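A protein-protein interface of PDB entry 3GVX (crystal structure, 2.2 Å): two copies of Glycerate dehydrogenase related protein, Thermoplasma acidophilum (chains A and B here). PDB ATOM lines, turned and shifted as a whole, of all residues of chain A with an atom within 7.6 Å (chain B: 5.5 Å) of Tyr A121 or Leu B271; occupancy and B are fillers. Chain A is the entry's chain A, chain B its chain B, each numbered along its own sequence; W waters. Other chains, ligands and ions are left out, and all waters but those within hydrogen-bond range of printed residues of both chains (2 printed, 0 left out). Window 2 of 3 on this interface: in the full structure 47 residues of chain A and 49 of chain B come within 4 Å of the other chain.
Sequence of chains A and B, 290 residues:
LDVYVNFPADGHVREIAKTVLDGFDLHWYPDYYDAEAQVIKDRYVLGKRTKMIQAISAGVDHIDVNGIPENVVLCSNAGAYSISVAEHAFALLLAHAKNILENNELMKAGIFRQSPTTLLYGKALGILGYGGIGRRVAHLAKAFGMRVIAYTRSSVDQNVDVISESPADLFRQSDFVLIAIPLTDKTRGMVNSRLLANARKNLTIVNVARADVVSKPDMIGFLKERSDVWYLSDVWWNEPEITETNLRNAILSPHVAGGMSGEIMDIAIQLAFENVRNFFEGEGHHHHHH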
ATOM      1  N   LYS A  98     -14.504  10.432 -31.188  1.00  0.00           N
ATOM      2  CA  LYS A  98     -15.540  10.718 -30.205  1.00  0.00           C
ATOM      3  C   LYS A  98     -16.541  11.799 -30.619  1.00  0.00           C
ATOM      4  O   LYS A  98     -17.331  12.248 -29.790  1.00  0.00           O
ATOM      5  CB  LYS A  98     -14.921  11.103 -28.857  1.00  0.00           C
ATOM      6  CG  LYS A  98     -13.835  10.163 -28.369  1.00  0.00           C
ATOM      7  CD  LYS A  98     -14.189   8.689 -28.537  1.00  0.00           C
ATOM      8  CE  LYS A  98     -13.089   7.833 -27.919  1.00  0.00           C
ATOM      9  NZ  LYS A  98     -13.161   6.377 -28.199  1.00  0.00           N
ATOM     10  N   THR A 118     -16.510   6.043 -31.814  1.00  0.00           N
ATOM     11  CA  THR A 118     -15.611   5.008 -32.286  1.00  0.00           C
ATOM     12  C   THR A 118     -14.578   4.788 -31.196  1.00  0.00           C
ATOM     13  O   THR A 118     -14.062   5.726 -30.586  1.00  0.00           O
ATOM     14  CB  THR A 118     -14.911   5.436 -33.580  1.00  0.00           C
ATOM     15  OG1 THR A 118     -15.902   5.656 -34.582  1.00  0.00           O
ATOM     16  CG2 THR A 118     -13.938   4.370 -34.060  1.00  0.00           C
ATOM     17  N   LEU A 119     -14.286   3.531 -30.939  1.00  0.00           N
ATOM     18  CA  LEU A 119     -13.320   3.204 -29.919  1.00  0.00           C
ATOM     19  C   LEU A 119     -11.990   2.883 -30.609  1.00  0.00           C
ATOM     20  O   LEU A 119     -11.974   2.258 -31.667  1.00  0.00           O
ATOM     21  CB  LEU A 119     -13.849   2.018 -29.114  1.00  0.00           C
ATOM     22  CG  LEU A 119     -13.024   1.511 -27.941  1.00  0.00           C
ATOM     23  CD1 LEU A 119     -13.416   2.196 -26.613  1.00  0.00           C
ATOM     24  CD2 LEU A 119     -13.241   0.009 -27.893  1.00  0.00           C
ATOM     25  N   LEU A 120     -10.879   3.331 -30.028  1.00  0.00           N
ATOM     26  CA  LEU A 120      -9.570   3.080 -30.634  1.00  0.00           C
ATOM     27  C   LEU A 120      -9.086   1.688 -30.297  1.00  0.00           C
ATOM     28  O   LEU A 120      -8.546   0.978 -31.136  1.00  0.00           O
ATOM     29  CB  LEU A 120      -8.541   4.085 -30.136  1.00  0.00           C
ATOM     30  CG  LEU A 120      -8.799   5.560 -30.431  1.00  0.00           C
ATOM     31  CD1 LEU A 120      -7.552   6.331 -30.036  1.00  0.00           C
ATOM     32  CD2 LEU A 120      -9.148   5.768 -31.908  1.00  0.00           C
ATOM     33  N   TYR A 121      -9.297   1.316 -29.042  1.00  0.00           N
ATOM     34  CA  TYR A 121      -8.898   0.017 -28.536  1.00  0.00           C
ATOM     35  C   TYR A 121      -9.299  -1.115 -29.476  1.00  0.00           C
ATOM     36  O   TYR A 121     -10.462  -1.224 -29.855  1.00  0.00           O
ATOM     37  CB  TYR A 121      -9.532  -0.219 -27.165  1.00  0.00           C
ATOM     38  CG  TYR A 121      -9.028  -1.459 -26.490  1.00  0.00           C
ATOM     39  CD1 TYR A 121      -8.036  -1.387 -25.528  1.00  0.00           C
ATOM     40  CD2 TYR A 121      -9.530  -2.724 -26.824  1.00  0.00           C
ATOM     41  CE1 TYR A 121      -7.542  -2.536 -24.909  1.00  0.00           C
ATOM     42  CE2 TYR A 121      -9.036  -3.888 -26.211  1.00  0.00           C
ATOM     43  CZ  TYR A 121      -8.050  -3.785 -25.251  1.00  0.00           C
ATOM     44  OH  TYR A 121      -7.580  -4.913 -24.616  1.00  0.00           O
ATOM     45  N   GLY A 122      -8.337  -1.956 -29.846  1.00  0.00           N
ATOM     46  CA  GLY A 122      -8.618  -3.075 -30.729  1.00  0.00           C
ATOM     47  C   GLY A 122      -8.589  -2.784 -32.223  1.00  0.00           C
ATOM     48  O   GLY A 122      -8.797  -3.673 -33.044  1.00  0.00           O
ATOM     49  N   LYS A 123      -8.311  -1.546 -32.595  1.00  0.00           N
ATOM     50  CA  LYS A 123      -8.278  -1.207 -34.005  1.00  0.00           C
ATOM     51  C   LYS A 123      -6.888  -1.162 -34.604  1.00  0.00           C
ATOM     52  O   LYS A 123      -5.887  -1.218 -33.894  1.00  0.00           O
ATOM     53  CB  LYS A 123      -9.006   0.112 -34.236  1.00  0.00           C
ATOM     54  CG  LYS A 123     -10.477   0.053 -33.859  1.00  0.00           C
ATOM     55  CD  LYS A 123     -11.368   0.043 -35.087  1.00  0.00           C
ATOM     56  CE  LYS A 123     -12.600   0.877 -34.818  1.00  0.00           C
ATOM     57  NZ  LYS A 123     -13.390   0.317 -33.689  1.00  0.00           N
ATOM     58  N   ALA A 124      -6.843  -1.047 -35.924  1.00  0.00           N
ATOM     59  CA  ALA A 124      -5.584  -1.003 -36.636  1.00  0.00           C
ATOM     60  C   ALA A 124      -5.184   0.374 -37.160  1.00  0.00           C
ATOM     61  O   ALA A 124      -5.912   1.021 -37.920  1.00  0.00           O
ATOM     62  CB  ALA A 124      -5.606  -2.009 -37.792  1.00  0.00           C
ATOM     63  N   ALA A 141      -0.174   4.482 -29.760  1.00  0.00           N
ATOM     64  CA  ALA A 141      -1.116   3.513 -30.295  1.00  0.00           C
ATOM     65  C   ALA A 141      -1.129   2.207 -29.495  1.00  0.00           C
ATOM     66  O   ALA A 141      -2.180   1.733 -29.095  1.00  0.00           O
ATOM     67  CB  ALA A 141      -0.794   3.254 -31.759  1.00  0.00           C
ATOM     68  N   LYS A 142       0.043   1.647 -29.234  1.00  0.00           N
ATOM     69  CA  LYS A 142       0.102   0.418 -28.452  1.00  0.00           C
ATOM     70  C   LYS A 142      -0.500   0.633 -27.069  1.00  0.00           C
ATOM     71  O   LYS A 142      -1.189  -0.235 -26.543  1.00  0.00           O
ATOM     72  CB  LYS A 142       1.546  -0.081 -28.336  1.00  0.00           C
ATOM     73  CG  LYS A 142       2.234  -0.387 -29.683  1.00  0.00           C
ATOM     74  CD  LYS A 142       1.468  -1.408 -30.530  1.00  0.00           C
ATOM     75  CE  LYS A 142       1.054  -2.635 -29.714  1.00  0.00           C
ATOM     76  NZ  LYS A 142       0.197  -3.589 -30.487  1.00  0.00           N
ATOM     77  N   ALA A 143      -0.257   1.800 -26.483  1.00  0.00           N
ATOM     78  CA  ALA A 143      -0.811   2.117 -25.169  1.00  0.00           C
ATOM     79  C   ALA A 143      -2.336   2.142 -25.241  1.00  0.00           C
ATOM     80  O   ALA A 143      -3.023   1.703 -24.329  1.00  0.00           O
ATOM     81  CB  ALA A 143      -0.282   3.463 -24.670  1.00  0.00           C
ATOM     82  N   PHE A 144      -2.855   2.642 -26.351  1.00  0.00           N
ATOM     83  CA  PHE A 144      -4.296   2.702 -26.558  1.00  0.00           C
ATOM     84  C   PHE A 144      -4.832   1.316 -26.922  1.00  0.00           C
ATOM     85  O   PHE A 144      -6.034   1.117 -27.027  1.00  0.00           O
ATOM     86  CB  PHE A 144      -4.634   3.707 -27.666  1.00  0.00           C
ATOM     87  CG  PHE A 144      -4.923   5.097 -27.170  1.00  0.00           C
ATOM     88  CD1 PHE A 144      -6.165   5.436 -26.678  1.00  0.00           C
ATOM     89  CD2 PHE A 144      -3.950   6.072 -27.197  1.00  0.00           C
ATOM     90  CE1 PHE A 144      -6.420   6.729 -26.225  1.00  0.00           C
ATOM     91  CE2 PHE A 144      -4.208   7.357 -26.742  1.00  0.00           C
ATOM     92  CZ  PHE A 144      -5.439   7.677 -26.259  1.00  0.00           C
ATOM     93  N   GLY A 145      -3.927   0.366 -27.126  1.00  0.00           N
ATOM     94  CA  GLY A 145      -4.343  -0.977 -27.470  1.00  0.00           C
ATOM     95  C   GLY A 145      -4.668  -1.143 -28.935  1.00  0.00           C
ATOM     96  O   GLY A 145      -5.527  -1.916 -29.297  1.00  0.00           O
ATOM     97  N   MET A 146      -3.975  -0.418 -29.791  1.00  0.00           N
ATOM     98  CA  MET A 146      -4.201  -0.533 -31.215  1.00  0.00           C
ATOM     99  C   MET A 146      -3.155  -1.448 -31.815  1.00  0.00           C
ATOM    100  O   MET A 146      -2.115  -1.710 -31.234  1.00  0.00           O
ATOM    101  CB  MET A 146      -4.114   0.847 -31.876  1.00  0.00           C
ATOM    102  CG  MET A 146      -5.065   1.869 -31.294  1.00  0.00           C
ATOM    103  SD  MET A 146      -4.838   3.494 -32.025  1.00  0.00           S
ATOM    104  CE  MET A 146      -6.005   3.536 -33.187  1.00  0.00           C
ATOM    105  N   ARG A 147      -3.441  -1.919 -33.007  1.00  0.00           N
ATOM    106  CA  ARG A 147      -2.496  -2.730 -33.724  1.00  0.00           C
ATOM    107  C   ARG A 147      -1.804  -1.765 -34.675  1.00  0.00           C
ATOM    108  O   ARG A 147      -2.440  -0.868 -35.228  1.00  0.00           O
ATOM    109  CB  ARG A 147      -3.234  -3.802 -34.493  1.00  0.00           C
ATOM    110  CG  ARG A 147      -2.416  -4.545 -35.500  1.00  0.00           C
ATOM    111  CD  ARG A 147      -3.260  -5.741 -35.895  1.00  0.00           C
ATOM    112  NE  ARG A 147      -2.666  -6.605 -36.907  1.00  0.00           N
ATOM    113  CZ  ARG A 147      -1.769  -7.550 -36.667  1.00  0.00           C
ATOM    114  NH1 ARG A 147      -1.331  -7.767 -35.436  1.00  0.00           N
ATOM    115  NH2 ARG A 147      -1.340  -8.303 -37.664  1.00  0.00           N
ATOM    116  N   PHE A 176      -7.293   3.334 -39.328  1.00  0.00           N
ATOM    117  CA  PHE A 176      -6.781   4.694 -39.251  1.00  0.00           C
ATOM    118  C   PHE A 176      -5.464   4.714 -39.995  1.00  0.00           C
ATOM    119  O   PHE A 176      -4.750   3.711 -40.054  1.00  0.00           O
ATOM    120  CB  PHE A 176      -6.529   5.126 -37.799  1.00  0.00           C
ATOM    121  CG  PHE A 176      -7.736   5.054 -36.916  1.00  0.00           C
ATOM    122  CD1 PHE A 176      -8.583   6.144 -36.764  1.00  0.00           C
ATOM    123  CD2 PHE A 176      -8.038   3.887 -36.242  1.00  0.00           C
ATOM    124  CE1 PHE A 176      -9.703   6.063 -35.955  1.00  0.00           C
ATOM    125  CE2 PHE A 176      -9.155   3.804 -35.444  1.00  0.00           C
ATOM    126  CZ  PHE A 176      -9.988   4.896 -35.299  1.00  0.00           C
ATOM    127  N   ASN B  77     -17.147  -8.904 -16.479  1.00  0.00           N
ATOM    128  CA  ASN B  77     -16.396  -8.314 -17.585  1.00  0.00           C
ATOM    129  C   ASN B  77     -16.689  -6.820 -17.782  1.00  0.00           C
ATOM    130  O   ASN B  77     -17.514  -6.456 -18.611  1.00  0.00           O
ATOM    131  CB  ASN B  77     -16.738  -9.119 -18.838  1.00  0.00           C
ATOM    132  CG  ASN B  77     -15.999  -8.661 -20.062  1.00  0.00           C
ATOM    133  OD1 ASN B  77     -14.797  -8.404 -20.021  1.00  0.00           O
ATOM    134  ND2 ASN B  77     -16.711  -8.589 -21.181  1.00  0.00           N
ATOM    135  N   GLY B  79     -14.024  -4.337 -18.170  1.00  0.00           N
ATOM    136  CA  GLY B  79     -12.923  -3.606 -18.761  1.00  0.00           C
ATOM    137  C   GLY B  79     -13.236  -2.648 -19.895  1.00  0.00           C
ATOM    138  O   GLY B  79     -12.661  -1.563 -19.937  1.00  0.00           O
ATOM    139  N   ALA B  80     -14.141  -3.032 -20.798  1.00  0.00           N
ATOM    140  CA  ALA B  80     -14.503  -2.210 -21.956  1.00  0.00           C
ATOM    141  C   ALA B  80     -14.996  -0.829 -21.563  1.00  0.00           C
ATOM    142  O   ALA B  80     -14.693   0.175 -22.205  1.00  0.00           O
ATOM    143  CB  ALA B  80     -15.564  -2.919 -22.803  1.00  0.00           C
ATOM    144  N   ILE B  83     -12.050   1.377 -20.338  1.00  0.00           N
ATOM    145  CA  ILE B  83     -11.214   1.597 -21.517  1.00  0.00           C
ATOM    146  C   ILE B  83     -11.836   2.724 -22.335  1.00  0.00           C
ATOM    147  O   ILE B  83     -11.180   3.699 -22.701  1.00  0.00           O
ATOM    148  CB  ILE B  83     -11.143   0.328 -22.398  1.00  0.00           C
ATOM    149  CG1 ILE B  83     -10.182  -0.674 -21.761  1.00  0.00           C
ATOM    150  CG2 ILE B  83     -10.789   0.696 -23.843  1.00  0.00           C
ATOM    151  CD1 ILE B  83     -10.155  -2.023 -22.432  1.00  0.00           C
ATOM    152  N   GLU B  87     -10.534   6.725 -22.861  1.00  0.00           N
ATOM    153  CA  GLU B  87     -10.328   7.234 -24.221  1.00  0.00           C
ATOM    154  C   GLU B  87     -11.124   8.503 -24.464  1.00  0.00           C
ATOM    155  O   GLU B  87     -10.665   9.413 -25.145  1.00  0.00           O
ATOM    156  CB  GLU B  87     -10.732   6.205 -25.271  1.00  0.00           C
ATOM    157  CG  GLU B  87      -9.736   5.107 -25.538  1.00  0.00           C
ATOM    158  CD  GLU B  87     -10.167   4.228 -26.712  1.00  0.00           C
ATOM    159  OE1 GLU B  87     -10.933   4.710 -27.566  1.00  0.00           O
ATOM    160  OE2 GLU B  87      -9.750   3.061 -26.796  1.00  0.00           O
ATOM    161  N   ARG B 136      -7.121   3.146 -15.692  1.00  0.00           N
ATOM    162  CA  ARG B 136      -6.982   3.134 -17.135  1.00  0.00           C
ATOM    163  C   ARG B 136      -6.503   4.492 -17.634  1.00  0.00           C
ATOM    164  O   ARG B 136      -5.698   4.573 -18.539  1.00  0.00           O
ATOM    165  CB  ARG B 136      -8.312   2.769 -17.787  1.00  0.00           C
ATOM    166  CG  ARG B 136      -8.235   2.615 -19.284  1.00  0.00           C
ATOM    167  CD  ARG B 136      -7.215   1.568 -19.712  1.00  0.00           C
ATOM    168  NE  ARG B 136      -7.124   1.503 -21.167  1.00  0.00           N
ATOM    169  CZ  ARG B 136      -6.376   0.655 -21.863  1.00  0.00           C
ATOM    170  NH1 ARG B 136      -5.621  -0.237 -21.245  1.00  0.00           N
ATOM    171  NH2 ARG B 136      -6.400   0.710 -23.190  1.00  0.00           N
ATOM    172  N   ILE B 267     -15.851  -5.399 -28.424  1.00  0.00           N
ATOM    173  CA  ILE B 267     -14.639  -5.721 -27.739  1.00  0.00           C
ATOM    174  C   ILE B 267     -14.860  -6.434 -26.396  1.00  0.00           C
ATOM    175  O   ILE B 267     -13.972  -7.136 -25.908  1.00  0.00           O
ATOM    176  CB  ILE B 267     -13.835  -4.403 -27.635  1.00  0.00           C
ATOM    177  CG1 ILE B 267     -12.505  -4.576 -28.371  1.00  0.00           C
ATOM    178  CG2 ILE B 267     -13.791  -3.888 -26.208  1.00  0.00           C
ATOM    179  CD1 ILE B 267     -11.786  -5.895 -28.117  1.00  0.00           C
ATOM    180  N   ALA B 268     -16.053  -6.267 -25.825  1.00  0.00           N
ATOM    181  CA  ALA B 268     -16.416  -6.887 -24.547  1.00  0.00           C
ATOM    182  C   ALA B 268     -16.274  -8.402 -24.582  1.00  0.00           C
ATOM    183  O   ALA B 268     -15.657  -8.990 -23.706  1.00  0.00           O
ATOM    184  CB  ALA B 268     -17.845  -6.499 -24.162  1.00  0.00           C
ATOM    185  N   ILE B 269     -16.810  -9.028 -25.623  1.00  0.00           N
ATOM    186  CA  ILE B 269     -16.742 -10.478 -25.733  1.00  0.00           C
ATOM    187  C   ILE B 269     -15.315 -11.013 -25.760  1.00  0.00           C
ATOM    188  O   ILE B 269     -15.025 -12.038 -25.157  1.00  0.00           O
ATOM    189  CB  ILE B 269     -17.577 -10.989 -26.953  1.00  0.00           C
ATOM    190  CG1 ILE B 269     -17.765 -12.508 -26.842  1.00  0.00           C
ATOM    191  CG2 ILE B 269     -16.959 -10.535 -28.272  1.00  0.00           C
ATOM    192  CD1 ILE B 269     -18.628 -12.923 -25.641  1.00  0.00           C
ATOM    193  N   GLN B 270     -14.406 -10.298 -26.415  1.00  0.00           N
ATOM    194  CA  GLN B 270     -13.015 -10.736 -26.462  1.00  0.00           C
ATOM    195  C   GLN B 270     -12.347 -10.637 -25.108  1.00  0.00           C
ATOM    196  O   GLN B 270     -11.605 -11.524 -24.711  1.00  0.00           O
ATOM    197  CB  GLN B 270     -12.220  -9.916 -27.465  1.00  0.00           C
ATOM    198  CG  GLN B 270     -10.843 -10.475 -27.731  1.00  0.00           C
ATOM    199  CD  GLN B 270     -10.162  -9.770 -28.880  1.00  0.00           C
ATOM    200  OE1 GLN B 270     -10.796  -9.454 -29.889  1.00  0.00           O
ATOM    201  NE2 GLN B 270      -8.867  -9.524 -28.740  1.00  0.00           N
ATOM    202  N   LEU B 271     -12.602  -9.538 -24.410  1.00  0.00           N
ATOM    203  CA  LEU B 271     -12.034  -9.335 -23.078  1.00  0.00           C
ATOM    204  C   LEU B 271     -12.535 -10.432 -22.136  1.00  0.00           C
ATOM    205  O   LEU B 271     -11.801 -10.887 -21.260  1.00  0.00           O
ATOM    206  CB  LEU B 271     -12.405  -7.944 -22.537  1.00  0.00           C
ATOM    207  CG  LEU B 271     -11.795  -6.749 -23.294  1.00  0.00           C
ATOM    208  CD1 LEU B 271     -12.539  -5.467 -22.927  1.00  0.00           C
ATOM    209  CD2 LEU B 271     -10.295  -6.652 -22.991  1.00  0.00           C
ATOM    210  N   ALA B 272     -13.783 -10.858 -22.334  1.00  0.00           N
ATOM    211  CA  ALA B 272     -14.371 -11.920 -21.518  1.00  0.00           C
ATOM    212  C   ALA B 272     -13.568 -13.209 -21.681  1.00  0.00           C
ATOM    213  O   ALA B 272     -13.151 -13.807 -20.698  1.00  0.00           O
ATOM    214  CB  ALA B 272     -15.846 -12.143 -21.901  1.00  0.00           C
ATOM    215  N   PHE B 273     -13.318 -13.624 -22.918  1.00  0.00           N
ATOM    216  CA  PHE B 273     -12.543 -14.850 -23.139  1.00  0.00           C
ATOM    217  C   PHE B 273     -11.117 -14.720 -22.660  1.00  0.00           C
ATOM    218  O   PHE B 273     -10.529 -15.668 -22.145  1.00  0.00           O
ATOM    219  CB  PHE B 273     -12.519 -15.254 -24.625  1.00  0.00           C
ATOM    220  CG  PHE B 273     -13.848 -15.690 -25.166  1.00  0.00           C
ATOM    221  CD1 PHE B 273     -14.640 -16.588 -24.478  1.00  0.00           C
ATOM    222  CD2 PHE B 273     -14.316 -15.195 -26.361  1.00  0.00           C
ATOM    223  CE1 PHE B 273     -15.875 -16.973 -24.970  1.00  0.00           C
ATOM    224  CE2 PHE B 273     -15.543 -15.584 -26.851  1.00  0.00           C
ATOM    225  CZ  PHE B 273     -16.320 -16.471 -26.150  1.00  0.00           C
ATOM    226  N   GLU B 274     -10.558 -13.536 -22.844  1.00  0.00           N
ATOM    227  CA  GLU B 274      -9.202 -13.282 -22.420  1.00  0.00           C
ATOM    228  C   GLU B 274      -9.061 -13.440 -20.924  1.00  0.00           C
ATOM    229  O   GLU B 274      -8.083 -14.011 -20.456  1.00  0.00           O
ATOM    230  CB  GLU B 274      -8.745 -11.896 -22.875  1.00  0.00           C
ATOM    231  CG  GLU B 274      -8.404 -11.883 -24.351  1.00  0.00           C
ATOM    232  CD  GLU B 274      -7.922 -10.530 -24.869  1.00  0.00           C
ATOM    233  OE1 GLU B 274      -8.284  -9.487 -24.293  1.00  0.00           O
ATOM    234  OE2 GLU B 274      -7.183 -10.507 -25.872  1.00  0.00           O
ATOM    235  N   ASN B 275     -10.044 -12.969 -20.169  1.00  0.00           N
ATOM    236  CA  ASN B 275      -9.955 -13.123 -18.730  1.00  0.00           C
ATOM    237  C   ASN B 275      -9.973 -14.590 -18.355  1.00  0.00           C
ATOM    238  O   ASN B 275      -9.398 -14.975 -17.352  1.00  0.00           O
ATOM    239  CB  ASN B 275     -11.089 -12.417 -17.991  1.00  0.00           C
ATOM    240  CG  ASN B 275     -10.808 -12.298 -16.505  1.00  0.00           C
ATOM    241  OD1 ASN B 275     -11.618 -12.694 -15.664  1.00  0.00           O
ATOM    242  ND2 ASN B 275      -9.644 -11.747 -16.176  1.00  0.00           N
ATOM    243  N   VAL B 276     -10.652 -15.404 -19.155  1.00  0.00           N
ATOM    244  CA  VAL B 276     -10.721 -16.840 -18.902  1.00  0.00           C
ATOM    245  C   VAL B 276      -9.342 -17.467 -19.041  1.00  0.00           C
ATOM    246  O   VAL B 276      -8.913 -18.271 -18.221  1.00  0.00           O
ATOM    247  CB  VAL B 276     -11.694 -17.529 -19.880  1.00  0.00           C
ATOM    248  CG1 VAL B 276     -11.443 -19.039 -19.885  1.00  0.00           C
ATOM    249  CG2 VAL B 276     -13.142 -17.204 -19.496  1.00  0.00           C
HETATM  250  O   HOH W   1      -7.632   2.369 -25.247  1.00  0.00           O
HETATM  251  O   HOH W   2      -4.119  -1.193 -23.815  1.00  0.00           O
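The side-chain carboxylate (OE1) of Glu B87 lies within salt-bridge range of the side-chain amino group (NZ) of Lys A98.
OE1 of Glu B87 sits at hydrogen-bond distance from N of Leu A120 (2.8 Å).
The backbone NH (N) of Tyr A121 is in hydrogen-bond range of the side-chain carboxylate (OE2) of Glu B87, at 2.9 Å.
The side-chain amino group of Lys A98 sits at hydrogen-bond distance from the backbone carbonyl oxygen of Thr A118 (2.6 Å).
NZ of Lys A123 lies within hydrogen-bond range of O of Leu A119, at 3.1 Å.
Leu A119 touches Glu B87 (CD1 to OE1, 3.7 Å).
Tyr A121 touches Ile B83.
CD1 of Tyr A121 touches NH2 of Arg B136, at 3.5 Å.
Ile B267 touches Tyr A121 (CG1 to CD2, 3.8 Å).
Tyr A121 touches Leu B271.
Ala A143 touches Arg B136 (O to NH2, 3.7 Å).
Phe A144 touches Glu B87.
Arg B136 touches Phe A144.
Tyr A121 touches five residues of chain B.
Of the printed residues of chain A, Ile B267 touches Tyr A121.
Of the printed residues of chain B, Leu A119 touches Glu B87.
Of the printed residues of chain A, Ile B83 touches Tyr A121.
Printed residues of chain A within 4 Å of Glu B87: Lys A98 (2.9 Å), Leu A119 (3.7 Å), Leu A120 (2.8 Å), Tyr A121 (2.9 Å) and Phe A144 (3.8 Å).
Lys A142 touches none of the printed residues of chain B.
Thr A118 touches none of the printed residues of chain B.
The nearest printed residue of chain B that does not touch Ala A143 is Glu B87 (7.3 Å).
Among the printed residues, 11 pairs touch across the chains.
Among the printed residues, Asp or Glu carboxylates within 4 Å of a Lys or Arg side-chain nitrogen of the other chain: Lys A98 with Glu B87.
No position is printed for both chains.
Water W1 lies within hydrogen-bond range of the backbone carbonyl oxygen (O) of Phe A144 (2.7 Å), the side-chain carboxylate (OE2) of Glu B87 (2.7 Å) and the guanidinium group (NH2) of Arg B136 (2.9 Å).
Water W2 lies within hydrogen-bond range of the guanidinium group (NH2) of Arg B136 (3.0 Å) and the backbone carbonyl oxygen (O) of Ala A143 (3.1 Å).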
